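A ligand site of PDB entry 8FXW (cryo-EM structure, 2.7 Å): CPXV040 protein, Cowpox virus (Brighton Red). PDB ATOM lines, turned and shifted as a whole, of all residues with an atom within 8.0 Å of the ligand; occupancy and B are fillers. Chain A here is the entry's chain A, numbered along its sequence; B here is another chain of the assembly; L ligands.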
ATOM      1  N   ARG A  18     -20.662 -20.645  22.529  1.00  0.00           N
ATOM      2  CA  ARG A  18     -21.358 -20.388  21.271  1.00  0.00           C
ATOM      3  C   ARG A  18     -21.374 -21.604  20.362  1.00  0.00           C
ATOM      4  O   ARG A  18     -22.322 -21.765  19.582  1.00  0.00           O
ATOM      5  CB  ARG A  18     -20.704 -19.207  20.548  1.00  0.00           C
ATOM      6  CG  ARG A  18     -20.845 -17.890  21.286  1.00  0.00           C
ATOM      7  CD  ARG A  18     -20.475 -16.706  20.403  1.00  0.00           C
ATOM      8  NE  ARG A  18     -19.043 -16.614  20.166  1.00  0.00           N
ATOM      9  CZ  ARG A  18     -18.190 -15.908  20.911  1.00  0.00           C
ATOM     10  NH1 ARG A  18     -18.600 -15.228  21.970  1.00  0.00           N
ATOM     11  NH2 ARG A  18     -16.904 -15.897  20.584  1.00  0.00           N
ATOM     12  N   TYR A  19     -20.358 -22.454  20.435  1.00  0.00           N
ATOM     13  CA  TYR A  19     -20.238 -23.615  19.574  1.00  0.00           C
ATOM     14  C   TYR A  19     -20.668 -24.850  20.355  1.00  0.00           C
ATOM     15  O   TYR A  19     -20.063 -25.190  21.375  1.00  0.00           O
ATOM     16  CB  TYR A  19     -18.810 -23.771  19.063  1.00  0.00           C
ATOM     17  CG  TYR A  19     -18.310 -22.555  18.311  1.00  0.00           C
ATOM     18  CD1 TYR A  19     -17.867 -21.431  18.997  1.00  0.00           C
ATOM     19  CD2 TYR A  19     -18.307 -22.530  16.925  1.00  0.00           C
ATOM     20  CE1 TYR A  19     -17.421 -20.320  18.313  1.00  0.00           C
ATOM     21  CE2 TYR A  19     -17.861 -21.419  16.242  1.00  0.00           C
ATOM     22  CZ  TYR A  19     -17.417 -20.319  16.933  1.00  0.00           C
ATOM     23  OH  TYR A  19     -16.979 -19.210  16.256  1.00  0.00           O
ATOM     24  N   HIS A 159     -31.688 -28.816  15.583  1.00  0.00           N
ATOM     25  CA  HIS A 159     -31.857 -27.411  15.263  1.00  0.00           C
ATOM     26  C   HIS A 159     -33.171 -26.881  15.825  1.00  0.00           C
ATOM     27  O   HIS A 159     -33.198 -25.775  16.374  1.00  0.00           O
ATOM     28  CB  HIS A 159     -31.769 -27.193  13.755  1.00  0.00           C
ATOM     29  CG  HIS A 159     -30.364 -27.272  13.235  1.00  0.00           C
ATOM     30  ND1 HIS A 159     -29.407 -26.335  13.545  1.00  0.00           N
ATOM     31  CD2 HIS A 159     -29.765 -28.179  12.428  1.00  0.00           C
ATOM     32  CE1 HIS A 159     -28.273 -26.659  12.951  1.00  0.00           C
ATOM     33  NE2 HIS A 159     -28.453 -27.779  12.265  1.00  0.00           N
ATOM     34  N   HIS A 162     -33.401 -23.620  17.019  1.00  0.00           N
ATOM     35  CA  HIS A 162     -31.972 -23.450  17.270  1.00  0.00           C
ATOM     36  C   HIS A 162     -31.703 -22.022  17.757  1.00  0.00           C
ATOM     37  O   HIS A 162     -32.144 -21.061  17.103  1.00  0.00           O
ATOM     38  CB  HIS A 162     -31.189 -23.741  15.990  1.00  0.00           C
ATOM     39  CG  HIS A 162     -29.803 -23.181  15.980  1.00  0.00           C
ATOM     40  ND1 HIS A 162     -28.963 -23.237  17.078  1.00  0.00           N
ATOM     41  CD2 HIS A 162     -29.090 -22.572  14.997  1.00  0.00           C
ATOM     42  CE1 HIS A 162     -27.806 -22.674  16.776  1.00  0.00           C
ATOM     43  NE2 HIS A 162     -27.859 -22.261  15.517  1.00  0.00           N
ATOM     44  N   PRO A 163     -30.999 -21.846  18.875  1.00  0.00           N
ATOM     45  CA  PRO A 163     -30.726 -20.474  19.340  1.00  0.00           C
ATOM     46  C   PRO A 163     -29.983 -19.682  18.280  1.00  0.00           C
ATOM     47  O   PRO A 163     -29.118 -20.194  17.575  1.00  0.00           O
ATOM     48  CB  PRO A 163     -29.875 -20.698  20.593  1.00  0.00           C
ATOM     49  CG  PRO A 163     -30.232 -22.051  21.059  1.00  0.00           C
ATOM     50  CD  PRO A 163     -30.512 -22.853  19.820  1.00  0.00           C
ATOM     51  N   LYS A 164     -30.339 -18.393  18.173  1.00  0.00           N
ATOM     52  CA  LYS A 164     -29.867 -17.595  17.055  1.00  0.00           C
ATOM     53  C   LYS A 164     -28.380 -17.275  17.179  1.00  0.00           C
ATOM     54  O   LYS A 164     -27.674 -17.148  16.165  1.00  0.00           O
ATOM     55  CB  LYS A 164     -30.678 -16.304  16.959  1.00  0.00           C
ATOM     56  CG  LYS A 164     -30.324 -15.416  15.783  1.00  0.00           C
ATOM     57  CD  LYS A 164     -30.592 -16.093  14.449  1.00  0.00           C
ATOM     58  CE  LYS A 164     -30.282 -15.187  13.277  1.00  0.00           C
ATOM     59  NZ  LYS A 164     -31.123 -13.950  13.287  1.00  0.00           N
ATOM     60  N   ASP A 165     -27.876 -17.129  18.398  1.00  0.00           N
ATOM     61  CA  ASP A 165     -26.507 -16.667  18.607  1.00  0.00           C
ATOM     62  C   ASP A 165     -25.483 -17.789  18.582  1.00  0.00           C
ATOM     63  O   ASP A 165     -24.290 -17.499  18.739  1.00  0.00           O
ATOM     64  CB  ASP A 165     -26.425 -15.923  19.937  1.00  0.00           C
ATOM     65  CG  ASP A 165     -27.385 -14.759  20.031  1.00  0.00           C
ATOM     66  OD1 ASP A 165     -28.126 -14.525  19.042  1.00  0.00           O
ATOM     67  OD2 ASP A 165     -27.418 -14.085  21.080  1.00  0.00           O
ATOM     68  N   LYS A 166     -25.896 -19.037  18.383  1.00  0.00           N
ATOM     69  CA  LYS A 166     -25.007 -20.180  18.528  1.00  0.00           C
ATOM     70  C   LYS A 166     -24.756 -20.855  17.184  1.00  0.00           C
ATOM     71  O   LYS A 166     -25.382 -20.551  16.171  1.00  0.00           O
ATOM     72  CB  LYS A 166     -25.589 -21.189  19.508  1.00  0.00           C
ATOM     73  CG  LYS A 166     -26.247 -20.600  20.733  1.00  0.00           C
ATOM     74  CD  LYS A 166     -25.253 -19.933  21.656  1.00  0.00           C
ATOM     75  CE  LYS A 166     -25.926 -19.459  22.926  1.00  0.00           C
ATOM     76  NZ  LYS A 166     -24.968 -18.810  23.862  1.00  0.00           N
ATOM     77  N   TYR A 167     -23.811 -21.783  17.198  1.00  0.00           N
ATOM     78  CA  TYR A 167     -23.540 -22.689  16.091  1.00  0.00           C
ATOM     79  C   TYR A 167     -23.728 -24.110  16.589  1.00  0.00           C
ATOM     80  O   TYR A 167     -23.272 -24.438  17.693  1.00  0.00           O
ATOM     81  CB  TYR A 167     -22.118 -22.499  15.548  1.00  0.00           C
ATOM     82  CG  TYR A 167     -21.744 -21.064  15.261  1.00  0.00           C
ATOM     83  CD1 TYR A 167     -21.417 -20.197  16.286  1.00  0.00           C
ATOM     84  CD2 TYR A 167     -21.709 -20.585  13.959  1.00  0.00           C
ATOM     85  CE1 TYR A 167     -21.079 -18.884  16.032  1.00  0.00           C
ATOM     86  CE2 TYR A 167     -21.370 -19.282  13.701  1.00  0.00           C
ATOM     87  CZ  TYR A 167     -21.051 -18.442  14.738  1.00  0.00           C
ATOM     88  OH  TYR A 167     -20.704 -17.135  14.474  1.00  0.00           O
ATOM     89  N   LEU A 168     -24.418 -24.933  15.812  1.00  0.00           N
ATOM     90  CA  LEU A 168     -24.739 -26.298  16.199  1.00  0.00           C
ATOM     91  C   LEU A 168     -24.063 -27.291  15.266  1.00  0.00           C
ATOM     92  O   LEU A 168     -24.016 -27.074  14.059  1.00  0.00           O
ATOM     93  CB  LEU A 168     -26.252 -26.532  16.183  1.00  0.00           C
ATOM     94  CG  LEU A 168     -27.015 -26.257  17.481  1.00  0.00           C
ATOM     95  CD1 LEU A 168     -28.502 -26.329  17.219  1.00  0.00           C
ATOM     96  CD2 LEU A 168     -26.619 -27.245  18.556  1.00  0.00           C
ATOM     97  N   TYR A 169     -23.542 -28.369  15.850  1.00  0.00           N
ATOM     98  CA  TYR A 169     -22.928 -29.443  15.086  1.00  0.00           C
ATOM     99  C   TYR A 169     -23.474 -30.770  15.593  1.00  0.00           C
ATOM    100  O   TYR A 169     -23.817 -30.913  16.759  1.00  0.00           O
ATOM    101  CB  TYR A 169     -21.400 -29.417  15.227  1.00  0.00           C
ATOM    102  CG  TYR A 169     -20.802 -28.066  14.917  1.00  0.00           C
ATOM    103  CD1 TYR A 169     -20.538 -27.681  13.611  1.00  0.00           C
ATOM    104  CD2 TYR A 169     -20.498 -27.170  15.944  1.00  0.00           C
ATOM    105  CE1 TYR A 169     -19.995 -26.450  13.325  1.00  0.00           C
ATOM    106  CE2 TYR A 169     -19.955 -25.940  15.658  1.00  0.00           C
ATOM    107  CZ  TYR A 169     -19.704 -25.587  14.354  1.00  0.00           C
ATOM    108  OH  TYR A 169     -19.148 -24.357  14.069  1.00  0.00           O
ATOM    109  N   ASP B  33     -16.361 -21.549  11.850  1.00  0.00           N
ATOM    110  CA  ASP B  33     -17.265 -20.558  11.292  1.00  0.00           C
ATOM    111  C   ASP B  33     -17.339 -19.313  12.168  1.00  0.00           C
ATOM    112  O   ASP B  33     -17.560 -19.411  13.377  1.00  0.00           O
ATOM    113  CB  ASP B  33     -18.663 -21.169  11.129  1.00  0.00           C
ATOM    114  CG  ASP B  33     -18.683 -22.319  10.162  1.00  0.00           C
ATOM    115  OD1 ASP B  33     -18.066 -23.357  10.464  1.00  0.00           O
ATOM    116  OD2 ASP B  33     -19.322 -22.190   9.101  1.00  0.00           O
ATOM    117  N   ILE B  34     -17.155 -18.154  11.543  1.00  0.00           N
ATOM    118  CA  ILE B  34     -17.522 -16.872  12.112  1.00  0.00           C
ATOM    119  C   ILE B  34     -18.391 -16.174  11.075  1.00  0.00           C
ATOM    120  O   ILE B  34     -18.009 -16.089   9.896  1.00  0.00           O
ATOM    121  CB  ILE B  34     -16.298 -16.005  12.476  1.00  0.00           C
ATOM    122  CG1 ILE B  34     -15.150 -16.885  12.976  1.00  0.00           C
ATOM    123  CG2 ILE B  34     -16.674 -14.989  13.534  1.00  0.00           C
ATOM    124  CD1 ILE B  34     -13.911 -16.099  13.356  1.00  0.00           C
ATOM    125  N   ASN B  35     -19.549 -15.669  11.502  1.00  0.00           N
ATOM    126  CA  ASN B  35     -20.561 -15.228  10.550  1.00  0.00           C
ATOM    127  C   ASN B  35     -20.495 -13.728  10.272  1.00  0.00           C
ATOM    128  O   ASN B  35     -20.352 -13.316   9.127  1.00  0.00           O
ATOM    129  CB  ASN B  35     -21.954 -15.621  11.068  1.00  0.00           C
ATOM    130  CG  ASN B  35     -22.501 -16.845  10.372  1.00  0.00           C
ATOM    131  OD1 ASN B  35     -23.521 -16.779   9.691  1.00  0.00           O
ATOM    132  ND2 ASN B  35     -21.812 -17.970  10.524  1.00  0.00           N
ATOM    133  N   SER B  36     -20.587 -12.914  11.311  1.00  0.00           N
ATOM    134  CA  SER B  36     -20.662 -11.480  11.124  1.00  0.00           C
ATOM    135  C   SER B  36     -20.101 -10.762  12.345  1.00  0.00           C
ATOM    136  O   SER B  36     -19.912 -11.368  13.402  1.00  0.00           O
ATOM    137  CB  SER B  36     -22.098 -11.020  10.855  1.00  0.00           C
ATOM    138  OG  SER B  36     -22.935 -11.328  11.955  1.00  0.00           O
ATOM    139  N   ILE B  38     -20.044  -8.560  15.607  1.00  0.00           N
ATOM    140  CA  ILE B  38     -20.931  -8.481  16.757  1.00  0.00           C
ATOM    141  C   ILE B  38     -20.483  -7.318  17.619  1.00  0.00           C
ATOM    142  O   ILE B  38     -19.291  -7.163  17.898  1.00  0.00           O
ATOM    143  CB  ILE B  38     -20.935  -9.794  17.556  1.00  0.00           C
ATOM    144  CG1 ILE B  38     -21.432 -10.947  16.687  1.00  0.00           C
ATOM    145  CG2 ILE B  38     -21.791  -9.647  18.811  1.00  0.00           C
ATOM    146  CD1 ILE B  38     -21.293 -12.306  17.327  1.00  0.00           C
HETATM  147  C1  LIG L   1     -24.925 -18.717  11.382  1.00  0.00           C
HETATM  148  C2  LIG L   1     -25.434 -19.282  12.696  1.00  0.00           C
HETATM  149  C3  LIG L   1     -25.162 -20.787  12.763  1.00  0.00           C
HETATM  150  C4  LIG L   1     -25.722 -21.476  11.523  1.00  0.00           C
HETATM  151  C5  LIG L   1     -25.199 -20.801  10.261  1.00  0.00           C
HETATM  152  C6  LIG L   1     -25.817 -21.354   8.994  1.00  0.00           C
HETATM  153  C7  LIG L   1     -24.974 -17.308  14.070  1.00  0.00           C
HETATM  154  C8  LIG L   1     -24.273 -16.772  15.284  1.00  0.00           C
HETATM  155  N1  LIG L   1     -24.821 -18.612  13.826  1.00  0.00           N
HETATM  156  O1  LIG L   1     -25.765 -21.333  13.932  1.00  0.00           O
HETATM  157  O2  LIG L   1     -25.332 -22.847  11.515  1.00  0.00           O
HETATM  158  O3  LIG L   1     -25.527 -19.403  10.292  1.00  0.00           O
HETATM  159  O4  LIG L   1     -25.987 -20.347   8.014  1.00  0.00           O
HETATM  160  O5  LIG L   1     -25.651 -16.590  13.339  1.00  0.00           O
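A ring nitrogen (NE2) of His 162 is in hydrogen-bond range of an oxygen (O1) of the ligand. O of Lys 166 lies within hydrogen-bond range of O1 of the ligand (2.4 Å). OD1 of Asn 35 of chain B sits close to O3 of the ligand (3.4 Å).
The backbone carbonyl oxygen (O) of Arg 18 sits at hydrogen-bond distance from the backbone NH (N) of Tyr 167 (2.8 Å). O of Lys 166 lies within hydrogen-bond range of NE2 of His 162 (3.1 Å).
Merely in contact with the ligand: Tyr 167, Lys 164 and Asp 165. Hydrophobic or aromatic side chains that line the ligand: His 162 and Tyr 167. Within 4 Å of the ligand: His 162, Lys 164, Asp 165, Lys 166, Tyr 167 and Asn 35 of chain B.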
